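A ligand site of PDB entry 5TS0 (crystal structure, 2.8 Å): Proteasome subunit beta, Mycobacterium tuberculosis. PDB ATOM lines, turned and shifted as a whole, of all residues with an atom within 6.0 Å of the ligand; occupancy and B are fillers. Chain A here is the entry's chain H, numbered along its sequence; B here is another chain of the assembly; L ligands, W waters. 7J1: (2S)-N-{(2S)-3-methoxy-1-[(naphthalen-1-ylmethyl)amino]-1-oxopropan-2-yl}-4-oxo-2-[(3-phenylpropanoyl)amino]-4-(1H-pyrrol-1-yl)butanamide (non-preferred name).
The side-chain amide nitrogen (NE2) of Gln 22 lies within hydrogen-bond range of an oxygen (O30) of the ligand, at 2.6 Å. O of Gly 47 lies within hydrogen-bond range of N06 of the ligand. The side-chain hydroxyl (OG) of Ser 27 lies within hydrogen-bond range of an oxygen (O30) of the ligand. The backbone NH (N) of Thr 21 lies within hydrogen-bond range of an oxygen (O18) of the ligand. The backbone carbonyl oxygen (O) of Thr 21 sits at hydrogen-bond distance from a nitrogen (N03) of the ligand (2.8 Å). The side-chain carboxylate (OD2) of Asp 124 of chain B is in hydrogen-bond range of a nitrogen (N31) of the ligand (2.9 Å). The backbone NH (N) of Ala 49 sits at hydrogen-bond distance from an oxygen (O01) of the ligand (3.1 Å).
N of Ser 27 sits at hydrogen-bond distance from O of Ser 20, at 2.6 Å. N of Ala 126 of chain B lies within hydrogen-bond range of OD1 of Asp 124 of chain B (3.1 Å). The side-chain hydroxyl (OG1) of Thr 1 lies within hydrogen-bond range of the side-chain amino group (NZ) of Lys 33, 3.1 Å away. The backbone carbonyl oxygen (O) of Ala 180 is in hydrogen-bond range of the backbone NH (N) of Thr 1 (2.9 Å). O of Thr 1 is in hydrogen-bond range of N of Ser 141. The side-chain amino group of Lys 33 sits at hydrogen-bond distance from the backbone carbonyl oxygen of Arg 19 (2.8 Å). OH of Tyr 35 sits at hydrogen-bond distance from O of Arg 32. The backbone carbonyl oxygen (O) of Ser 122 of chain B is in hydrogen-bond range of the backbone NH (N) of Asn 130 of chain B (2.9 Å).
Thr 1 touches the ligand (OG1 to C07, 3.0 Å). Arg 19 touches the ligand (O to O18, 3.9 Å). Ser 20 touches the ligand. CG1 of Val 31 touches C15 of the ligand (3.6 Å). Arg 32 touches the ligand. Lys 33 touches the ligand (CG to C10, 3.6 Å). Ile 45 touches the ligand (O to C10, 3.4 Å). CA of Thr 48 touches O01 of the ligand, at 3.7 Å. CB of Ala 52 touches C10 of the ligand, at 3.8 Å. CD2 of Leu 98 touches C36 of the ligand (3.95 Å). CD1 of Leu 91 of chain B touches C37 of the ligand, at 3.6 Å. Met 95 of chain B touches the ligand (CE to C38, 3.5 Å). Ser 122 of chain B touches the ligand. Ala 126 of chain B touches the ligand (CB to C36, 3.8 Å). C of Gly 128 of chain B touches C28 of the ligand (3.6 Å). C of Trp 129 of chain B touches C28 of the ligand, 3.5 Å away. CB of Asn 130 of chain B touches C27 of the ligand, 3.8 Å away. Within 4 Å of the ligand: Thr 1, Arg 19, Ser 20, Thr 21, Gln 22, Ser 27, Val 31, Arg 32, Lys 33, Ile 45, Gly 47, Thr 48, Ala 49, Ala 52, Leu 98, Leu 91 of chain B, Met 95 of chain B, Ser 122 of chain B, Asp 124 of chain B, Ala 126 of chain B, Gly 128 of chain B, Trp 129 of chain B and Asn 130 of chain B.
Water W1 lies within hydrogen-bond range of the side-chain carboxylate (OD2) of Asp 124 of chain B, an oxygen (O01) of the ligand, the backbone NH (N) of Ala 49 and the backbone NH (N) of Ala 50.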
ATOM      1  N   THR A   1      10.979  12.782  21.411  1.00  0.00           N
ATOM      2  CA  THR A   1      10.981  11.351  21.702  1.00  0.00           C
ATOM      3  C   THR A   1      12.155  10.969  22.606  1.00  0.00           C
ATOM      4  O   THR A   1      13.275  11.418  22.368  1.00  0.00           O
ATOM      5  CB  THR A   1      11.134  10.529  20.417  1.00  0.00           C
ATOM      6  OG1 THR A   1      10.043  10.798  19.529  1.00  0.00           O
ATOM      7  CG2 THR A   1      11.154   9.040  20.753  1.00  0.00           C
ATOM      8  N   ARG A  19       4.758  11.263  23.531  1.00  0.00           N
ATOM      9  CA  ARG A  19       4.482  12.508  22.825  1.00  0.00           C
ATOM     10  C   ARG A  19       4.802  12.419  21.343  1.00  0.00           C
ATOM     11  O   ARG A  19       5.823  11.878  20.942  1.00  0.00           O
ATOM     12  CB  ARG A  19       5.262  13.671  23.436  1.00  0.00           C
ATOM     13  CG  ARG A  19       5.178  14.937  22.613  1.00  0.00           C
ATOM     14  CD  ARG A  19       5.582  16.141  23.407  1.00  0.00           C
ATOM     15  NE  ARG A  19       4.718  16.348  24.552  1.00  0.00           N
ATOM     16  CZ  ARG A  19       4.856  17.355  25.393  1.00  0.00           C
ATOM     17  NH1 ARG A  19       5.833  18.229  25.201  1.00  0.00           N
ATOM     18  NH2 ARG A  19       4.031  17.495  26.414  1.00  0.00           N
ATOM     19  N   SER A  20       3.890  12.958  20.534  1.00  0.00           N
ATOM     20  CA  SER A  20       4.021  13.120  19.089  1.00  0.00           C
ATOM     21  C   SER A  20       3.958  14.602  18.720  1.00  0.00           C
ATOM     22  O   SER A  20       3.068  15.320  19.190  1.00  0.00           O
ATOM     23  CB  SER A  20       2.908  12.366  18.386  1.00  0.00           C
ATOM     24  OG  SER A  20       2.744  12.811  17.073  1.00  0.00           O
ATOM     25  N   THR A  21       4.907  15.064  17.905  1.00  0.00           N
ATOM     26  CA  THR A  21       4.995  16.464  17.502  1.00  0.00           C
ATOM     27  C   THR A  21       5.093  16.610  15.982  1.00  0.00           C
ATOM     28  O   THR A  21       5.531  15.719  15.266  1.00  0.00           O
ATOM     29  CB  THR A  21       6.216  17.198  18.116  1.00  0.00           C
ATOM     30  OG1 THR A  21       7.388  16.400  17.944  1.00  0.00           O
ATOM     31  CG2 THR A  21       6.026  17.552  19.593  1.00  0.00           C
ATOM     32  N   GLN A  22       4.711  17.802  15.523  1.00  0.00           N
ATOM     33  CA  GLN A  22       4.941  18.264  14.155  1.00  0.00           C
ATOM     34  C   GLN A  22       5.568  19.640  14.308  1.00  0.00           C
ATOM     35  O   GLN A  22       4.868  20.641  14.445  1.00  0.00           O
ATOM     36  CB  GLN A  22       3.679  18.294  13.352  1.00  0.00           C
ATOM     37  CG  GLN A  22       3.303  16.929  12.889  1.00  0.00           C
ATOM     38  CD  GLN A  22       2.367  16.955  11.706  1.00  0.00           C
ATOM     39  OE1 GLN A  22       2.352  17.910  10.921  1.00  0.00           O
ATOM     40  NE2 GLN A  22       1.611  15.876  11.537  1.00  0.00           N
ATOM     41  N   GLY A  23       6.893  19.689  14.299  1.00  0.00           N
ATOM     42  CA  GLY A  23       7.586  20.885  14.674  1.00  0.00           C
ATOM     43  C   GLY A  23       7.451  21.119  16.151  1.00  0.00           C
ATOM     44  O   GLY A  23       7.843  20.285  16.970  1.00  0.00           O
ATOM     45  N   SER A  27       1.128  16.843  18.315  1.00  0.00           N
ATOM     46  CA  SER A  27       0.150  16.101  17.526  1.00  0.00           C
ATOM     47  C   SER A  27      -0.337  14.804  18.188  1.00  0.00           C
ATOM     48  O   SER A  27      -1.249  14.172  17.652  1.00  0.00           O
ATOM     49  CB  SER A  27       0.700  15.811  16.125  1.00  0.00           C
ATOM     50  OG  SER A  27       1.981  15.195  16.139  1.00  0.00           O
ATOM     51  N   VAL A  31       0.767   8.188  22.100  1.00  0.00           N
ATOM     52  CA  VAL A  31       1.372   7.302  21.107  1.00  0.00           C
ATOM     53  C   VAL A  31       2.226   6.262  21.824  1.00  0.00           C
ATOM     54  O   VAL A  31       2.686   6.469  22.960  1.00  0.00           O
ATOM     55  CB  VAL A  31       2.182   8.114  20.083  1.00  0.00           C
ATOM     56  CG1 VAL A  31       1.349   9.306  19.616  1.00  0.00           C
ATOM     57  CG2 VAL A  31       3.472   8.593  20.692  1.00  0.00           C
ATOM     58  N   ARG A  32       2.412   5.101  21.185  1.00  0.00           N
ATOM     59  CA  ARG A  32       3.211   4.025  21.747  1.00  0.00           C
ATOM     60  C   ARG A  32       4.466   3.857  20.896  1.00  0.00           C
ATOM     61  O   ARG A  32       4.391   3.802  19.667  1.00  0.00           O
ATOM     62  CB  ARG A  32       2.420   2.712  21.819  1.00  0.00           C
ATOM     63  CG  ARG A  32       1.110   2.876  22.645  1.00  0.00           C
ATOM     64  CD  ARG A  32       0.353   1.564  22.904  1.00  0.00           C
ATOM     65  NE  ARG A  32       0.645   1.013  24.238  1.00  0.00           N
ATOM     66  CZ  ARG A  32       1.412  -0.060  24.463  1.00  0.00           C
ATOM     67  NH1 ARG A  32       1.978  -0.732  23.451  1.00  0.00           N
ATOM     68  NH2 ARG A  32       1.624  -0.454  25.716  1.00  0.00           N
ATOM     69  N   LYS A  33       5.614   3.838  21.559  1.00  0.00           N
ATOM     70  CA  LYS A  33       6.882   3.785  20.850  1.00  0.00           C
ATOM     71  C   LYS A  33       7.696   2.548  21.209  1.00  0.00           C
ATOM     72  O   LYS A  33       8.762   2.347  20.624  1.00  0.00           O
ATOM     73  CB  LYS A  33       7.696   5.055  21.129  1.00  0.00           C
ATOM     74  CG  LYS A  33       6.911   6.370  20.920  1.00  0.00           C
ATOM     75  CD  LYS A  33       7.756   7.562  21.338  1.00  0.00           C
ATOM     76  CE  LYS A  33       6.982   8.862  21.315  1.00  0.00           C
ATOM     77  NZ  LYS A  33       7.855  10.016  21.615  1.00  0.00           N
ATOM     78  N   TYR A  35       7.452  -1.715  21.511  1.00  0.00           N
ATOM     79  CA  TYR A  35       6.653  -2.844  21.054  1.00  0.00           C
ATOM     80  C   TYR A  35       7.295  -4.170  21.419  1.00  0.00           C
ATOM     81  O   TYR A  35       8.512  -4.331  21.331  1.00  0.00           O
ATOM     82  CB  TYR A  35       6.456  -2.820  19.536  1.00  0.00           C
ATOM     83  CG  TYR A  35       5.865  -1.541  19.042  1.00  0.00           C
ATOM     84  CD1 TYR A  35       6.686  -0.467  18.719  1.00  0.00           C
ATOM     85  CD2 TYR A  35       4.490  -1.381  18.909  1.00  0.00           C
ATOM     86  CE1 TYR A  35       6.162   0.716  18.281  1.00  0.00           C
ATOM     87  CE2 TYR A  35       3.944  -0.201  18.462  1.00  0.00           C
ATOM     88  CZ  TYR A  35       4.803   0.852  18.150  1.00  0.00           C
ATOM     89  OH  TYR A  35       4.299   2.059  17.700  1.00  0.00           O
ATOM     90  N   ILE A  45      11.354   2.630  18.894  1.00  0.00           N
ATOM     91  CA  ILE A  45      11.846   3.339  17.719  1.00  0.00           C
ATOM     92  C   ILE A  45      11.581   4.834  17.879  1.00  0.00           C
ATOM     93  O   ILE A  45      10.538   5.239  18.407  1.00  0.00           O
ATOM     94  CB  ILE A  45      11.228   2.788  16.437  1.00  0.00           C
ATOM     95  CG1 ILE A  45      11.435   1.263  16.386  1.00  0.00           C
ATOM     96  CG2 ILE A  45      11.940   3.401  15.241  1.00  0.00           C
ATOM     97  CD1 ILE A  45      10.543   0.530  15.441  1.00  0.00           C
ATOM     98  N   ALA A  46      12.542   5.654  17.409  1.00  0.00           N
ATOM     99  CA  ALA A  46      12.467   7.106  17.395  1.00  0.00           C
ATOM    100  C   ALA A  46      12.531   7.609  15.961  1.00  0.00           C
ATOM    101  O   ALA A  46      13.141   6.977  15.109  1.00  0.00           O
ATOM    102  CB  ALA A  46      13.601   7.700  18.208  1.00  0.00           C
ATOM    103  N   GLY A  47      11.897   8.756  15.698  1.00  0.00           N
ATOM    104  CA  GLY A  47      11.935   9.371  14.382  1.00  0.00           C
ATOM    105  C   GLY A  47      10.545   9.561  13.807  1.00  0.00           C
ATOM    106  O   GLY A  47       9.569   9.761  14.543  1.00  0.00           O
ATOM    107  N   THR A  48      10.457   9.526  12.470  1.00  0.00           N
ATOM    108  CA  THR A  48       9.166   9.643  11.813  1.00  0.00           C
ATOM    109  C   THR A  48       8.239   8.491  12.197  1.00  0.00           C
ATOM    110  O   THR A  48       8.598   7.324  12.051  1.00  0.00           O
ATOM    111  CB  THR A  48       9.329   9.677  10.294  1.00  0.00           C
ATOM    112  OG1 THR A  48      10.623  10.186   9.958  1.00  0.00           O
ATOM    113  CG2 THR A  48       8.238  10.491   9.621  1.00  0.00           C
ATOM    114  N   ALA A  49       7.042   8.838  12.676  1.00  0.00           N
ATOM    115  CA  ALA A  49       6.123   7.834  13.202  1.00  0.00           C
ATOM    116  C   ALA A  49       5.794   6.770  12.151  1.00  0.00           C
ATOM    117  O   ALA A  49       5.856   5.570  12.438  1.00  0.00           O
ATOM    118  CB  ALA A  49       4.831   8.490  13.676  1.00  0.00           C
ATOM    119  N   ALA A  50       5.441   7.205  10.934  1.00  0.00           N
ATOM    120  CA  ALA A  50       5.085   6.256   9.893  1.00  0.00           C
ATOM    121  C   ALA A  50       6.185   5.215   9.688  1.00  0.00           C
ATOM    122  O   ALA A  50       5.945   4.001   9.727  1.00  0.00           O
ATOM    123  CB  ALA A  50       4.796   7.003   8.587  1.00  0.00           C
ATOM    124  N   ALA A  52       8.665   4.474  11.750  1.00  0.00           N
ATOM    125  CA  ALA A  52       8.910   3.716  12.974  1.00  0.00           C
ATOM    126  C   ALA A  52       7.888   2.581  13.150  1.00  0.00           C
ATOM    127  O   ALA A  52       8.255   1.442  13.473  1.00  0.00           O
ATOM    128  CB  ALA A  52       8.902   4.651  14.179  1.00  0.00           C
ATOM    129  N   VAL A  53       6.591   2.886  12.967  1.00  0.00           N
ATOM    130  CA  VAL A  53       5.582   1.845  13.150  1.00  0.00           C
ATOM    131  C   VAL A  53       5.746   0.772  12.097  1.00  0.00           C
ATOM    132  O   VAL A  53       5.666  -0.437  12.406  1.00  0.00           O
ATOM    133  CB  VAL A  53       4.156   2.441  13.179  1.00  0.00           C
ATOM    134  CG1 VAL A  53       3.074   1.383  12.972  1.00  0.00           C
ATOM    135  CG2 VAL A  53       3.952   3.101  14.532  1.00  0.00           C
ATOM    136  N   GLY A  97      14.523  12.553   4.803  1.00  0.00           N
ATOM    137  CA  GLY A  97      13.582  12.991   5.852  1.00  0.00           C
ATOM    138  C   GLY A  97      12.734  11.900   6.520  1.00  0.00           C
ATOM    139  O   GLY A  97      12.033  12.204   7.502  1.00  0.00           O
ATOM    140  N   LEU A  98      12.715  10.652   6.055  1.00  0.00           N
ATOM    141  CA  LEU A  98      11.951   9.591   6.702  1.00  0.00           C
ATOM    142  C   LEU A  98      12.863   8.747   7.607  1.00  0.00           C
ATOM    143  O   LEU A  98      12.915   7.512   7.496  1.00  0.00           O
ATOM    144  CB  LEU A  98      11.275   8.729   5.637  1.00  0.00           C
ATOM    145  CG  LEU A  98      10.281   9.535   4.796  1.00  0.00           C
ATOM    146  CD1 LEU A  98       9.493   8.709   3.762  1.00  0.00           C
ATOM    147  CD2 LEU A  98       9.330  10.283   5.728  1.00  0.00           C
ATOM    148  N   SER A 141      15.435  12.384  20.746  1.00  0.00           N
ATOM    149  CA  SER A 141      15.909  13.748  20.970  1.00  0.00           C
ATOM    150  C   SER A 141      16.271  14.034  22.423  1.00  0.00           C
ATOM    151  O   SER A 141      17.015  14.979  22.684  1.00  0.00           O
ATOM    152  CB  SER A 141      14.899  14.798  20.487  1.00  0.00           C
ATOM    153  OG  SER A 141      13.603  14.540  20.984  1.00  0.00           O
ATOM    154  N   ALA A 180      10.375  17.789  23.018  1.00  0.00           N
ATOM    155  CA  ALA A 180       9.831  16.740  22.159  1.00  0.00           C
ATOM    156  C   ALA A 180       9.545  15.438  22.897  1.00  0.00           C
ATOM    157  O   ALA A 180       8.896  14.546  22.332  1.00  0.00           O
ATOM    158  CB  ALA A 180      10.772  16.473  20.980  1.00  0.00           C
ATOM    159  N   LEU B  91       3.177   9.985  -1.413  1.00  0.00           N
ATOM    160  CA  LEU B  91       4.065  11.002  -0.827  1.00  0.00           C
ATOM    161  C   LEU B  91       4.934  11.718  -1.880  1.00  0.00           C
ATOM    162  O   LEU B  91       5.074  12.956  -1.836  1.00  0.00           O
ATOM    163  CB  LEU B  91       4.953  10.384   0.266  1.00  0.00           C
ATOM    164  CG  LEU B  91       6.024  11.298   0.913  1.00  0.00           C
ATOM    165  CD1 LEU B  91       5.392  12.521   1.509  1.00  0.00           C
ATOM    166  CD2 LEU B  91       6.866  10.575   1.974  1.00  0.00           C
ATOM    167  N   MET B  95       4.947  15.824  -2.244  1.00  0.00           N
ATOM    168  CA  MET B  95       6.092  16.736  -2.123  1.00  0.00           C
ATOM    169  C   MET B  95       6.250  17.642  -3.331  1.00  0.00           C
ATOM    170  O   MET B  95       6.953  18.657  -3.238  1.00  0.00           O
ATOM    171  CB  MET B  95       7.384  15.909  -1.977  1.00  0.00           C
ATOM    172  CG  MET B  95       7.592  15.156  -0.664  1.00  0.00           C
ATOM    173  SD  MET B  95       7.886  16.248   0.753  1.00  0.00           S
ATOM    174  CE  MET B  95       6.235  16.637   1.323  1.00  0.00           C
ATOM    175  N   SER B 122      -6.857   9.803  12.193  1.00  0.00           N
ATOM    176  CA  SER B 122      -6.241  10.904  11.467  1.00  0.00           C
ATOM    177  C   SER B 122      -4.916  10.430  10.888  1.00  0.00           C
ATOM    178  O   SER B 122      -4.318   9.482  11.401  1.00  0.00           O
ATOM    179  CB  SER B 122      -6.011  12.109  12.380  1.00  0.00           C
ATOM    180  OG  SER B 122      -5.161  11.729  13.452  1.00  0.00           O
ATOM    181  N   PHE B 123      -4.454  11.105   9.831  1.00  0.00           N
ATOM    182  CA  PHE B 123      -3.242  10.678   9.106  1.00  0.00           C
ATOM    183  C   PHE B 123      -2.278  11.842   8.888  1.00  0.00           C
ATOM    184  O   PHE B 123      -2.638  13.021   9.042  1.00  0.00           O
ATOM    185  CB  PHE B 123      -3.581  10.065   7.744  1.00  0.00           C
ATOM    186  CG  PHE B 123      -4.401   8.819   7.841  1.00  0.00           C
ATOM    187  CD1 PHE B 123      -5.771   8.882   7.979  1.00  0.00           C
ATOM    188  CD2 PHE B 123      -3.787   7.564   7.791  1.00  0.00           C
ATOM    189  CE1 PHE B 123      -6.507   7.715   8.069  1.00  0.00           C
ATOM    190  CE2 PHE B 123      -4.516   6.425   7.874  1.00  0.00           C
ATOM    191  CZ  PHE B 123      -5.880   6.492   8.020  1.00  0.00           C
ATOM    192  N   ASP B 124      -1.032  11.515   8.563  1.00  0.00           N
ATOM    193  CA  ASP B 124      -0.084  12.518   8.097  1.00  0.00           C
ATOM    194  C   ASP B 124       0.400  12.160   6.697  1.00  0.00           C
ATOM    195  O   ASP B 124       0.065  11.116   6.143  1.00  0.00           O
ATOM    196  CB  ASP B 124       1.091  12.697   9.088  1.00  0.00           C
ATOM    197  CG  ASP B 124       2.017  11.499   9.138  1.00  0.00           C
ATOM    198  OD1 ASP B 124       1.980  10.628   8.248  1.00  0.00           O
ATOM    199  OD2 ASP B 124       2.842  11.454  10.077  1.00  0.00           O
ATOM    200  N   ALA B 125       1.206  13.049   6.112  1.00  0.00           N
ATOM    201  CA  ALA B 125       1.575  12.927   4.707  1.00  0.00           C
ATOM    202  C   ALA B 125       2.360  11.657   4.389  1.00  0.00           C
ATOM    203  O   ALA B 125       2.360  11.224   3.228  1.00  0.00           O
ATOM    204  CB  ALA B 125       2.359  14.160   4.258  1.00  0.00           C
ATOM    205  N   ALA B 126       3.026  11.053   5.375  1.00  0.00           N
ATOM    206  CA  ALA B 126       3.773   9.806   5.216  1.00  0.00           C
ATOM    207  C   ALA B 126       2.928   8.565   5.446  1.00  0.00           C
ATOM    208  O   ALA B 126       3.468   7.455   5.437  1.00  0.00           O
ATOM    209  CB  ALA B 126       4.968   9.767   6.176  1.00  0.00           C
ATOM    210  N   GLY B 128       1.631   7.759   8.348  1.00  0.00           N
ATOM    211  CA  GLY B 128       1.434   7.685   9.779  1.00  0.00           C
ATOM    212  C   GLY B 128      -0.022   7.887  10.129  1.00  0.00           C
ATOM    213  O   GLY B 128      -0.699   8.727   9.502  1.00  0.00           O
ATOM    214  N   TRP B 129      -0.553   7.124  11.094  1.00  0.00           N
ATOM    215  CA  TRP B 129      -1.940   7.268  11.507  1.00  0.00           C
ATOM    216  C   TRP B 129      -2.039   7.277  13.025  1.00  0.00           C
ATOM    217  O   TRP B 129      -1.174   6.772  13.730  1.00  0.00           O
ATOM    218  CB  TRP B 129      -2.797   6.152  10.925  1.00  0.00           C
ATOM    219  CG  TRP B 129      -2.189   4.789  11.095  1.00  0.00           C
ATOM    220  CD1 TRP B 129      -1.356   4.147  10.215  1.00  0.00           C
ATOM    221  CD2 TRP B 129      -2.354   3.907  12.203  1.00  0.00           C
ATOM    222  NE1 TRP B 129      -1.013   2.920  10.706  1.00  0.00           N
ATOM    223  CE2 TRP B 129      -1.610   2.744  11.923  1.00  0.00           C
ATOM    224  CE3 TRP B 129      -3.064   3.967  13.399  1.00  0.00           C
ATOM    225  CZ2 TRP B 129      -1.548   1.670  12.791  1.00  0.00           C
ATOM    226  CZ3 TRP B 129      -3.008   2.889  14.260  1.00  0.00           C
ATOM    227  CH2 TRP B 129      -2.254   1.767  13.952  1.00  0.00           C
ATOM    228  N   ASN B 130      -3.161   7.806  13.502  1.00  0.00           N
ATOM    229  CA  ASN B 130      -3.486   7.874  14.920  1.00  0.00           C
ATOM    230  C   ASN B 130      -4.962   7.569  15.102  1.00  0.00           C
ATOM    231  O   ASN B 130      -5.810   8.250  14.517  1.00  0.00           O
ATOM    232  CB  ASN B 130      -3.141   9.260  15.472  1.00  0.00           C
ATOM    233  CG  ASN B 130      -3.882   9.596  16.755  1.00  0.00           C
ATOM    234  OD1 ASN B 130      -3.965   8.804  17.707  1.00  0.00           O
ATOM    235  ND2 ASN B 130      -4.465  10.809  16.766  1.00  0.00           N
HETATM  236  C32 7J1 L   1       5.156  14.216  10.762  1.00  0.00           C
HETATM  237  O41 7J1 L   1       5.957  14.920  11.322  1.00  0.00           O
HETATM  238  C33 7J1 L   1       5.023  14.246   9.250  1.00  0.00           C
HETATM  239  C34 7J1 L   1       6.274  13.761   8.529  1.00  0.00           C
HETATM  240  C35 7J1 L   1       6.312  14.126   7.080  1.00  0.00           C
HETATM  241  C36 7J1 L   1       6.670  13.186   6.100  1.00  0.00           C
HETATM  242  C37 7J1 L   1       6.698  13.540   4.757  1.00  0.00           C
HETATM  243  C38 7J1 L   1       6.359  14.837   4.371  1.00  0.00           C
HETATM  244  C39 7J1 L   1       6.002  15.777   5.337  1.00  0.00           C
HETATM  245  C40 7J1 L   1       5.975  15.423   6.666  1.00  0.00           C
HETATM  246  N31 7J1 L   1       4.379  13.385  11.548  1.00  0.00           N
HETATM  247  C22 7J1 L   1       4.508  13.371  12.988  1.00  0.00           C
HETATM  248  C23 7J1 L   1       3.431  12.503  13.682  1.00  0.00           C
HETATM  249  C24 7J1 L   1       2.072  13.042  13.483  1.00  0.00           C
HETATM  250  O30 7J1 L   1       1.863  14.241  13.523  1.00  0.00           O
HETATM  251  N25 7J1 L   1       1.016  12.192  13.241  1.00  0.00           N
HETATM  252  C29 7J1 L   1       1.036  10.733  13.165  1.00  0.00           C
HETATM  253  C28 7J1 L   1      -0.405  10.325  12.768  1.00  0.00           C
HETATM  254  C26 7J1 L   1      -0.364  12.740  13.026  1.00  0.00           C
HETATM  255  C27 7J1 L   1      -1.298  11.525  13.105  1.00  0.00           C
HETATM  256  C02 7J1 L   1       5.852  12.728  13.371  1.00  0.00           C
HETATM  257  O01 7J1 L   1       6.393  11.871  12.685  1.00  0.00           O
HETATM  258  O20 7J1 L   1       9.744  13.696  14.991  1.00  0.00           O
HETATM  259  N03 7J1 L   1       6.430  13.124  14.538  1.00  0.00           N
HETATM  260  C04 7J1 L   1       7.611  12.633  15.032  1.00  0.00           C
HETATM  261  C05 7J1 L   1       7.272  11.806  16.336  1.00  0.00           C
HETATM  262  O18 7J1 L   1       6.331  12.147  17.052  1.00  0.00           O
HETATM  263  C19 7J1 L   1       8.432  13.891  15.418  1.00  0.00           C
HETATM  264  C21 7J1 L   1      10.613  13.193  16.009  1.00  0.00           C
HETATM  265  C11 7J1 L   1       6.108   5.860  17.098  1.00  0.00           C
HETATM  266  C10 7J1 L   1       7.406   6.022  17.405  1.00  0.00           C
HETATM  267  C12 7J1 L   1       5.278   6.973  17.001  1.00  0.00           C
HETATM  268  C14 7J1 L   1       4.899   9.337  17.084  1.00  0.00           C
HETATM  269  C13 7J1 L   1       5.786   8.251  17.208  1.00  0.00           C
HETATM  270  C15 7J1 L   1       3.595   9.122  16.770  1.00  0.00           C
HETATM  271  N06 7J1 L   1       7.996  10.660  16.629  1.00  0.00           N
HETATM  272  C07 7J1 L   1       7.747   9.834  17.778  1.00  0.00           C
HETATM  273  C08 7J1 L   1       7.148   8.431  17.514  1.00  0.00           C
HETATM  274  C09 7J1 L   1       7.931   7.312  17.620  1.00  0.00           C
HETATM  275  C16 7J1 L   1       3.096   7.815  16.572  1.00  0.00           C
HETATM  276  C17 7J1 L   1       3.928   6.763  16.675  1.00  0.00           C
HETATM  277  O   HOH W   1       5.229  10.517  10.640  1.00  0.00           O
